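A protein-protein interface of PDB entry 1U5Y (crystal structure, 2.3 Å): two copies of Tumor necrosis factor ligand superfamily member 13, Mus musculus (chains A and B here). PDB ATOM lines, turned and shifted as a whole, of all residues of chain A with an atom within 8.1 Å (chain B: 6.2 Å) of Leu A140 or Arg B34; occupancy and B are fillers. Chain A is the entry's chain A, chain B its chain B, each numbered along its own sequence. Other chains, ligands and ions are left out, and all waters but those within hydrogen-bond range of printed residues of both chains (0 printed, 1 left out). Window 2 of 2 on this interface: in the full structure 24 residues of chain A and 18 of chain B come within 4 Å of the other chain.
His A5 touches its own counterpart, His B5. Leu A140 touches His B5, but with the chains exchanged His A5 does not touch Leu B140 (7.0 Å). Leu A140 touches Val B138, but with the chains exchanged Val A138 does not touch Leu B140 (8.2 Å). 4 positions are printed for both chains.
His A5 touches His B5. Arg B34 touches Ile A52 (CZ to CD1, 3.95 Å). Val A106 touches Leu B32. Val A106 touches Val B138. Leu B32 touches Phe A107. His A108 touches Leu B32. Leu A140 touches His B5. CD1 of Leu A140 touches CG2 of Val B138, at 3.6 Å.
The guanidinium group (NH2) of Arg B34 lies within salt-bridge range of the chain-end carboxylate (O) of Leu A140 (3.0 Å).
Of the 13 printed residues of chain B, 4 touch a printed residue of chain A. Hydrophobic or aromatic side chains of chain B that line the printed part of chain A: His B5, Leu B32 and Val B138. Along chain B the printed residues that touch a printed residue of chain A span positions 5 to 138. Of the 16 printed residues of chain A, 6 touch a printed residue of chain B. Printed residues of chain A that touch a printed residue of chain B: His A5, Ile A52, Val A106, Phe A107, His A108 and Leu A140. Hydrophobic or aromatic side chains of chain A that line the printed part of chain B: His A5, Ile A52, Val A106 and Leu A140. Among the printed residues, no Asp or Glu carboxylate lies within 4 Å of a Lys or Arg side-chain nitrogen of the other chain.
ND1 of His A5 lies within hydrogen-bond range of O of Lys A139 (2.5 Å). The backbone carbonyl oxygen of Ile A52 is in hydrogen-bond range of the backbone NH of Leu A140, 2.8 Å away. The backbone NH (N) of Phe A107 lies within hydrogen-bond range of the backbone carbonyl oxygen (O) of Tyr A53, 3.0 Å away. NE of Arg B34 sits at hydrogen-bond distance from O of His B5, at 2.6 Å. The side-chain hydroxyl (OG) of Ser B6 lies within hydrogen-bond range of the backbone carbonyl oxygen (O) of Arg B34 (2.9 Å). The backbone NH (N) of Val B7 sits at hydrogen-bond distance from the backbone carbonyl oxygen (O) of Arg B34 (2.9 Å).
Of chain B, only His B5 (3.3 Å), Arg B34 (3.0 Å) and Val B138 (3.6 Å) come within 4 Å of Leu A140. Of chain A, only Ile A52 and Leu A140 come within 4 Å of Arg B34. Of the printed residues of chain A, His B5 touches His A5 and Leu A140. Printed residues of chain B within 4 Å of Phe A107: Leu B32. Lys A139 touches none of the printed residues of chain B. The nearest printed residue of chain B that does not touch Leu A140 is Val B7 (4.7 Å). The nearest printed residue of chain B that does not touch His A108 is Arg B34 (6.9 Å).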
ATOM      1  N   HIS A   5      11.730   4.944 -40.184  1.00  0.00           N
ATOM      2  CA  HIS A   5      10.598   4.331 -39.445  1.00  0.00           C
ATOM      3  C   HIS A   5       9.373   4.014 -40.335  1.00  0.00           C
ATOM      4  O   HIS A   5       8.996   4.828 -41.163  1.00  0.00           O
ATOM      5  CB  HIS A   5      10.089   5.305 -38.347  1.00  0.00           C
ATOM      6  CG  HIS A   5      11.091   5.656 -37.277  1.00  0.00           C
ATOM      7  ND1 HIS A   5      10.795   5.559 -35.931  1.00  0.00           N
ATOM      8  CD2 HIS A   5      12.349   6.158 -37.343  1.00  0.00           C
ATOM      9  CE1 HIS A   5      11.834   5.959 -35.220  1.00  0.00           C
ATOM     10  NE2 HIS A   5      12.792   6.323 -36.053  1.00  0.00           N
ATOM     11  N   SER A   6       8.717   2.873 -40.142  1.00  0.00           N
ATOM     12  CA  SER A   6       7.419   2.653 -40.795  1.00  0.00           C
ATOM     13  C   SER A   6       6.298   3.561 -40.189  1.00  0.00           C
ATOM     14  O   SER A   6       6.223   3.777 -38.983  1.00  0.00           O
ATOM     15  CB  SER A   6       7.029   1.169 -40.760  1.00  0.00           C
ATOM     16  OG  SER A   6       5.629   0.986 -40.573  1.00  0.00           O
ATOM     17  N   THR A  50       6.617  -6.942 -35.945  1.00  0.00           N
ATOM     18  CA  THR A  50       6.639  -6.923 -34.501  1.00  0.00           C
ATOM     19  C   THR A  50       7.485  -5.770 -34.003  1.00  0.00           C
ATOM     20  O   THR A  50       8.529  -5.495 -34.546  1.00  0.00           O
ATOM     21  CB  THR A  50       7.223  -8.244 -34.005  1.00  0.00           C
ATOM     22  OG1 THR A  50       6.371  -9.310 -34.422  1.00  0.00           O
ATOM     23  CG2 THR A  50       7.255  -8.317 -32.460  1.00  0.00           C
ATOM     24  N   GLY A  51       7.014  -5.091 -32.969  1.00  0.00           N
ATOM     25  CA  GLY A  51       7.752  -3.980 -32.410  1.00  0.00           C
ATOM     26  C   GLY A  51       6.901  -2.978 -31.661  1.00  0.00           C
ATOM     27  O   GLY A  51       5.723  -3.202 -31.361  1.00  0.00           O
ATOM     28  N   ILE A  52       7.534  -1.849 -31.370  1.00  0.00           N
ATOM     29  CA  ILE A  52       6.932  -0.803 -30.575  1.00  0.00           C
ATOM     30  C   ILE A  52       6.475   0.331 -31.454  1.00  0.00           C
ATOM     31  O   ILE A  52       7.220   0.802 -32.307  1.00  0.00           O
ATOM     32  CB  ILE A  52       7.912  -0.315 -29.521  1.00  0.00           C
ATOM     33  CG1 ILE A  52       8.271  -1.485 -28.589  1.00  0.00           C
ATOM     34  CG2 ILE A  52       7.299   0.897 -28.774  1.00  0.00           C
ATOM     35  CD1 ILE A  52       9.264  -1.144 -27.517  1.00  0.00           C
ATOM     36  N   TYR A  53       5.235   0.758 -31.220  1.00  0.00           N
ATOM     37  CA  TYR A  53       4.568   1.712 -32.057  1.00  0.00           C
ATOM     38  C   TYR A  53       3.894   2.789 -31.257  1.00  0.00           C
ATOM     39  O   TYR A  53       3.244   2.523 -30.253  1.00  0.00           O
ATOM     40  CB  TYR A  53       3.496   1.033 -32.857  1.00  0.00           C
ATOM     41  CG  TYR A  53       3.974   0.095 -33.922  1.00  0.00           C
ATOM     42  CD1 TYR A  53       3.974   0.485 -35.269  1.00  0.00           C
ATOM     43  CD2 TYR A  53       4.381  -1.206 -33.610  1.00  0.00           C
ATOM     44  CE1 TYR A  53       4.385  -0.407 -36.284  1.00  0.00           C
ATOM     45  CE2 TYR A  53       4.771  -2.092 -34.608  1.00  0.00           C
ATOM     46  CZ  TYR A  53       4.771  -1.680 -35.941  1.00  0.00           C
ATOM     47  OH  TYR A  53       5.148  -2.533 -36.930  1.00  0.00           O
ATOM     48  N   LEU A  54       4.055   4.019 -31.711  1.00  0.00           N
ATOM     49  CA  LEU A  54       3.163   5.085 -31.308  1.00  0.00           C
ATOM     50  C   LEU A  54       1.861   4.896 -32.090  1.00  0.00           C
ATOM     51  O   LEU A  54       1.855   4.767 -33.316  1.00  0.00           O
ATOM     52  CB  LEU A  54       3.801   6.419 -31.619  1.00  0.00           C
ATOM     53  CG  LEU A  54       3.000   7.707 -31.463  1.00  0.00           C
ATOM     54  CD1 LEU A  54       2.448   7.812 -30.083  1.00  0.00           C
ATOM     55  CD2 LEU A  54       3.916   8.886 -31.759  1.00  0.00           C
ATOM     56  N   LEU A  55       0.755   4.909 -31.380  1.00  0.00           N
ATOM     57  CA  LEU A  55      -0.548   4.747 -31.989  1.00  0.00           C
ATOM     58  C   LEU A  55      -1.439   5.909 -31.532  1.00  0.00           C
ATOM     59  O   LEU A  55      -1.563   6.151 -30.338  1.00  0.00           O
ATOM     60  CB  LEU A  55      -1.061   3.384 -31.568  1.00  0.00           C
ATOM     61  CG  LEU A  55      -2.462   2.882 -31.854  1.00  0.00           C
ATOM     62  CD1 LEU A  55      -3.017   3.418 -33.158  1.00  0.00           C
ATOM     63  CD2 LEU A  55      -2.438   1.328 -31.831  1.00  0.00           C
ATOM     64  N   GLY A 105      -0.911   6.537 -27.394  1.00  0.00           N
ATOM     65  CA  GLY A 105       0.051   5.923 -26.503  1.00  0.00           C
ATOM     66  C   GLY A 105       1.020   5.048 -27.258  1.00  0.00           C
ATOM     67  O   GLY A 105       0.885   4.850 -28.466  1.00  0.00           O
ATOM     68  N   VAL A 106       1.964   4.478 -26.529  1.00  0.00           N
ATOM     69  CA  VAL A 106       3.009   3.619 -27.094  1.00  0.00           C
ATOM     70  C   VAL A 106       2.829   2.185 -26.597  1.00  0.00           C
ATOM     71  O   VAL A 106       2.670   1.964 -25.391  1.00  0.00           O
ATOM     72  CB  VAL A 106       4.403   4.156 -26.732  1.00  0.00           C
ATOM     73  CG1 VAL A 106       5.496   3.285 -27.327  1.00  0.00           C
ATOM     74  CG2 VAL A 106       4.560   5.585 -27.254  1.00  0.00           C
ATOM     75  N   PHE A 107       2.853   1.223 -27.528  1.00  0.00           N
ATOM     76  CA  PHE A 107       2.538  -0.186 -27.240  1.00  0.00           C
ATOM     77  C   PHE A 107       3.298  -1.172 -28.080  1.00  0.00           C
ATOM     78  O   PHE A 107       3.637  -0.914 -29.227  1.00  0.00           O
ATOM     79  CB  PHE A 107       1.061  -0.460 -27.485  1.00  0.00           C
ATOM     80  CG  PHE A 107       0.163   0.486 -26.777  1.00  0.00           C
ATOM     81  CD1 PHE A 107      -0.235   1.662 -27.383  1.00  0.00           C
ATOM     82  CD2 PHE A 107      -0.281   0.201 -25.501  1.00  0.00           C
ATOM     83  CE1 PHE A 107      -1.076   2.564 -26.712  1.00  0.00           C
ATOM     84  CE2 PHE A 107      -1.120   1.102 -24.823  1.00  0.00           C
ATOM     85  CZ  PHE A 107      -1.501   2.274 -25.428  1.00  0.00           C
ATOM     86  N   HIS A 108       3.552  -2.322 -27.501  1.00  0.00           N
ATOM     87  CA  HIS A 108       4.200  -3.398 -28.209  1.00  0.00           C
ATOM     88  C   HIS A 108       3.131  -4.168 -28.993  1.00  0.00           C
ATOM     89  O   HIS A 108       2.186  -4.674 -28.406  1.00  0.00           O
ATOM     90  CB  HIS A 108       4.932  -4.305 -27.211  1.00  0.00           C
ATOM     91  CG  HIS A 108       5.886  -5.266 -27.849  1.00  0.00           C
ATOM     92  ND1 HIS A 108       5.597  -6.601 -28.008  1.00  0.00           N
ATOM     93  CD2 HIS A 108       7.128  -5.090 -28.353  1.00  0.00           C
ATOM     94  CE1 HIS A 108       6.618  -7.207 -28.585  1.00  0.00           C
ATOM     95  NE2 HIS A 108       7.559  -6.312 -28.807  1.00  0.00           N
ATOM     96  N   PHE A 137       0.061   5.505 -36.984  1.00  0.00           N
ATOM     97  CA  PHE A 137       1.050   4.604 -36.449  1.00  0.00           C
ATOM     98  C   PHE A 137       2.436   5.058 -36.828  1.00  0.00           C
ATOM     99  O   PHE A 137       2.682   5.398 -37.988  1.00  0.00           O
ATOM    100  CB  PHE A 137       0.875   3.204 -37.048  1.00  0.00           C
ATOM    101  CG  PHE A 137      -0.459   2.573 -36.771  1.00  0.00           C
ATOM    102  CD1 PHE A 137      -0.590   1.601 -35.788  1.00  0.00           C
ATOM    103  CD2 PHE A 137      -1.571   2.903 -37.545  1.00  0.00           C
ATOM    104  CE1 PHE A 137      -1.808   1.023 -35.547  1.00  0.00           C
ATOM    105  CE2 PHE A 137      -2.804   2.302 -37.319  1.00  0.00           C
ATOM    106  CZ  PHE A 137      -2.929   1.389 -36.313  1.00  0.00           C
ATOM    107  N   VAL A 138       3.356   5.004 -35.865  1.00  0.00           N
ATOM    108  CA  VAL A 138       4.776   5.151 -36.145  1.00  0.00           C
ATOM    109  C   VAL A 138       5.551   4.064 -35.417  1.00  0.00           C
ATOM    110  O   VAL A 138       5.471   3.969 -34.206  1.00  0.00           O
ATOM    111  CB  VAL A 138       5.301   6.519 -35.667  1.00  0.00           C
ATOM    112  CG1 VAL A 138       6.756   6.713 -36.111  1.00  0.00           C
ATOM    113  CG2 VAL A 138       4.426   7.633 -36.187  1.00  0.00           C
ATOM    114  N   LYS A 139       6.294   3.242 -36.144  1.00  0.00           N
ATOM    115  CA  LYS A 139       7.202   2.302 -35.505  1.00  0.00           C
ATOM    116  C   LYS A 139       8.355   3.079 -34.913  1.00  0.00           C
ATOM    117  O   LYS A 139       8.918   3.941 -35.579  1.00  0.00           O
ATOM    118  CB  LYS A 139       7.725   1.253 -36.477  1.00  0.00           C
ATOM    119  CG  LYS A 139       8.631   0.239 -35.792  1.00  0.00           C
ATOM    120  CD  LYS A 139       8.786  -1.054 -36.556  1.00  0.00           C
ATOM    121  CE  LYS A 139       9.633  -2.063 -35.762  1.00  0.00           C
ATOM    122  NZ  LYS A 139      10.258  -3.083 -36.631  1.00  0.00           N
ATOM    123  N   LEU A 140       8.702   2.757 -33.666  1.00  0.00           N
ATOM    124  CA  LEU A 140       9.655   3.536 -32.854  1.00  0.00           C
ATOM    125  C   LEU A 140      10.956   2.790 -32.610  1.00  0.00           C
ATOM    126  O   LEU A 140      11.852   3.338 -31.987  1.00  0.00           O
ATOM    127  CB  LEU A 140       9.050   3.851 -31.488  1.00  0.00           C
ATOM    128  CG  LEU A 140       7.893   4.834 -31.419  1.00  0.00           C
ATOM    129  CD1 LEU A 140       7.510   5.041 -29.939  1.00  0.00           C
ATOM    130  CD2 LEU A 140       8.272   6.134 -32.085  1.00  0.00           C
ATOM    131  OXT LEU A 140      11.172   1.641 -32.996  1.00  0.00           O
ATOM    132  N   LYS B   4      17.655   1.562 -31.792  1.00  0.00           N
ATOM    133  CA  LYS B   4      16.288   1.361 -31.213  1.00  0.00           C
ATOM    134  C   LYS B   4      16.021   2.326 -30.052  1.00  0.00           C
ATOM    135  O   LYS B   4      16.681   2.246 -29.009  1.00  0.00           O
ATOM    136  CB  LYS B   4      16.124  -0.083 -30.726  1.00  0.00           C
ATOM    137  CG  LYS B   4      16.376  -1.149 -31.793  1.00  0.00           C
ATOM    138  CD  LYS B   4      17.045  -2.398 -31.216  1.00  0.00           C
ATOM    139  CE  LYS B   4      17.367  -3.418 -32.314  1.00  0.00           C
ATOM    140  NZ  LYS B   4      17.908  -4.700 -31.778  1.00  0.00           N
ATOM    141  N   HIS B   5      15.029   3.203 -30.230  1.00  0.00           N
ATOM    142  CA  HIS B   5      14.681   4.264 -29.254  1.00  0.00           C
ATOM    143  C   HIS B   5      14.197   3.712 -27.881  1.00  0.00           C
ATOM    144  O   HIS B   5      13.422   2.759 -27.829  1.00  0.00           O
ATOM    145  CB  HIS B   5      13.574   5.181 -29.827  1.00  0.00           C
ATOM    146  CG  HIS B   5      13.980   5.982 -31.036  1.00  0.00           C
ATOM    147  ND1 HIS B   5      13.985   7.361 -31.045  1.00  0.00           N
ATOM    148  CD2 HIS B   5      14.362   5.601 -32.281  1.00  0.00           C
ATOM    149  CE1 HIS B   5      14.369   7.794 -32.232  1.00  0.00           C
ATOM    150  NE2 HIS B   5      14.603   6.746 -33.001  1.00  0.00           N
ATOM    151  N   SER B   6      14.661   4.342 -26.795  1.00  0.00           N
ATOM    152  CA  SER B   6      14.251   4.041 -25.415  1.00  0.00           C
ATOM    153  C   SER B   6      12.794   4.525 -25.112  1.00  0.00           C
ATOM    154  O   SER B   6      12.383   5.591 -25.570  1.00  0.00           O
ATOM    155  CB  SER B   6      15.247   4.709 -24.465  1.00  0.00           C
ATOM    156  OG  SER B   6      15.181   4.184 -23.144  1.00  0.00           O
ATOM    157  N   VAL B   7      12.006   3.728 -24.386  1.00  0.00           N
ATOM    158  CA  VAL B   7      10.594   4.060 -24.138  1.00  0.00           C
ATOM    159  C   VAL B   7      10.032   3.575 -22.804  1.00  0.00           C
ATOM    160  O   VAL B   7      10.554   2.675 -22.194  1.00  0.00           O
ATOM    161  CB  VAL B   7       9.659   3.593 -25.314  1.00  0.00           C
ATOM    162  CG1 VAL B   7      10.443   3.446 -26.634  1.00  0.00           C
ATOM    163  CG2 VAL B   7       8.930   2.320 -25.000  1.00  0.00           C
ATOM    164  N   LEU B   8       8.925   4.187 -22.388  1.00  0.00           N
ATOM    165  CA  LEU B   8       8.263   3.861 -21.137  1.00  0.00           C
ATOM    166  C   LEU B   8       6.777   4.201 -21.243  1.00  0.00           C
ATOM    167  O   LEU B   8       6.423   5.330 -21.564  1.00  0.00           O
ATOM    168  CB  LEU B   8       8.909   4.649 -20.005  1.00  0.00           C
ATOM    169  CG  LEU B   8       8.780   4.161 -18.573  1.00  0.00           C
ATOM    170  CD1 LEU B   8       9.359   2.774 -18.402  1.00  0.00           C
ATOM    171  CD2 LEU B   8       9.453   5.150 -17.654  1.00  0.00           C
ATOM    172  N   LEU B  32       5.450  -1.221 -20.090  1.00  0.00           N
ATOM    173  CA  LEU B  32       6.226  -1.378 -21.318  1.00  0.00           C
ATOM    174  C   LEU B  32       7.501  -0.618 -21.108  1.00  0.00           C
ATOM    175  O   LEU B  32       7.475   0.536 -20.724  1.00  0.00           O
ATOM    176  CB  LEU B  32       5.494  -0.808 -22.545  1.00  0.00           C
ATOM    177  CG  LEU B  32       6.317  -0.800 -23.842  1.00  0.00           C
ATOM    178  CD1 LEU B  32       6.711  -2.227 -24.258  1.00  0.00           C
ATOM    179  CD2 LEU B  32       5.549  -0.102 -24.956  1.00  0.00           C
ATOM    180  N   ARG B  33       8.613  -1.268 -21.382  1.00  0.00           N
ATOM    181  CA  ARG B  33       9.895  -0.700 -21.072  1.00  0.00           C
ATOM    182  C   ARG B  33      10.896  -1.126 -22.129  1.00  0.00           C
ATOM    183  O   ARG B  33      11.010  -2.319 -22.461  1.00  0.00           O
ATOM    184  CB  ARG B  33      10.333  -1.182 -19.691  1.00  0.00           C
ATOM    185  CG  ARG B  33      11.583  -0.526 -19.133  1.00  0.00           C
ATOM    186  CD  ARG B  33      11.884  -0.973 -17.701  1.00  0.00           C
ATOM    187  NE  ARG B  33      13.303  -0.979 -17.369  1.00  0.00           N
ATOM    188  CZ  ARG B  33      14.203  -1.854 -17.832  1.00  0.00           C
ATOM    189  NH1 ARG B  33      13.855  -2.809 -18.693  1.00  0.00           N
ATOM    190  NH2 ARG B  33      15.473  -1.766 -17.437  1.00  0.00           N
ATOM    191  N   ARG B  34      11.595  -0.140 -22.686  1.00  0.00           N
ATOM    192  CA  ARG B  34      12.781  -0.424 -23.483  1.00  0.00           C
ATOM    193  C   ARG B  34      13.869   0.544 -23.081  1.00  0.00           C
ATOM    194  O   ARG B  34      13.647   1.750 -23.069  1.00  0.00           O
ATOM    195  CB  ARG B  34      12.487  -0.296 -24.969  1.00  0.00           C
ATOM    196  CG  ARG B  34      13.735  -0.339 -25.828  1.00  0.00           C
ATOM    197  CD  ARG B  34      13.480  -0.791 -27.244  1.00  0.00           C
ATOM    198  NE  ARG B  34      12.931   0.269 -28.087  1.00  0.00           N
ATOM    199  CZ  ARG B  34      12.549   0.069 -29.349  1.00  0.00           C
ATOM    200  NH1 ARG B  34      12.606  -1.155 -29.885  1.00  0.00           N
ATOM    201  NH2 ARG B  34      12.083   1.079 -30.072  1.00  0.00           N
ATOM    202  N   GLY B  35      15.042   0.003 -22.751  1.00  0.00           N
ATOM    203  CA  GLY B  35      16.173   0.796 -22.305  1.00  0.00           C
ATOM    204  C   GLY B  35      16.032   1.119 -20.832  1.00  0.00           C
ATOM    205  O   GLY B  35      15.009   0.810 -20.217  1.00  0.00           O
ATOM    206  N   ARG B  36      17.059   1.755 -20.277  1.00  0.00           N
ATOM    207  CA  ARG B  36      17.135   2.041 -18.849  1.00  0.00           C
ATOM    208  C   ARG B  36      17.257   3.545 -18.572  1.00  0.00           C
ATOM    209  O   ARG B  36      17.553   3.946 -17.452  1.00  0.00           O
ATOM    210  CB  ARG B  36      18.349   1.323 -18.261  1.00  0.00           C
ATOM    211  CG  ARG B  36      18.307  -0.199 -18.331  1.00  0.00           C
ATOM    212  CD  ARG B  36      19.043  -0.857 -17.151  1.00  0.00           C
ATOM    213  NE  ARG B  36      19.312  -2.293 -17.293  1.00  0.00           N
ATOM    214  CZ  ARG B  36      18.668  -3.275 -16.639  1.00  0.00           C
ATOM    215  NH1 ARG B  36      17.672  -3.009 -15.796  1.00  0.00           N
ATOM    216  NH2 ARG B  36      19.020  -4.548 -16.837  1.00  0.00           N
ATOM    217  N   GLY B  37      17.021   4.380 -19.577  1.00  0.00           N
ATOM    218  CA  GLY B  37      17.223   5.808 -19.433  1.00  0.00           C
ATOM    219  C   GLY B  37      16.175   6.483 -18.570  1.00  0.00           C
ATOM    220  O   GLY B  37      16.339   7.635 -18.174  1.00  0.00           O
ATOM    221  N   VAL B 138       9.081   8.648 -24.930  1.00  0.00           N
ATOM    222  CA  VAL B 138       9.854   8.112 -26.043  1.00  0.00           C
ATOM    223  C   VAL B 138      11.040   9.027 -26.217  1.00  0.00           C
ATOM    224  O   VAL B 138      10.827  10.223 -26.462  1.00  0.00           O
ATOM    225  CB  VAL B 138       9.108   8.200 -27.404  1.00  0.00           C
ATOM    226  CG1 VAL B 138      10.007   7.645 -28.539  1.00  0.00           C
ATOM    227  CG2 VAL B 138       7.729   7.511 -27.373  1.00  0.00           C
ATOM    228  N   LEU B 140      13.846  10.611 -28.432  1.00  0.00           N
ATOM    229  CA  LEU B 140      13.914  10.909 -29.869  1.00  0.00           C
ATOM    230  C   LEU B 140      15.335  11.153 -30.336  1.00  0.00           C
ATOM    231  O   LEU B 140      15.552  11.248 -31.547  1.00  0.00           O
ATOM    232  CB  LEU B 140      13.090  12.157 -30.191  1.00  0.00           C
ATOM    233  CG  LEU B 140      11.641  12.123 -29.708  1.00  0.00           C
ATOM    234  CD1 LEU B 140      11.039  13.508 -29.834  1.00  0.00           C
ATOM    235  CD2 LEU B 140      10.860  11.079 -30.505  1.00  0.00           C
ATOM    236  OXT LEU B 140      16.242  11.264 -29.500  1.00  0.00           O
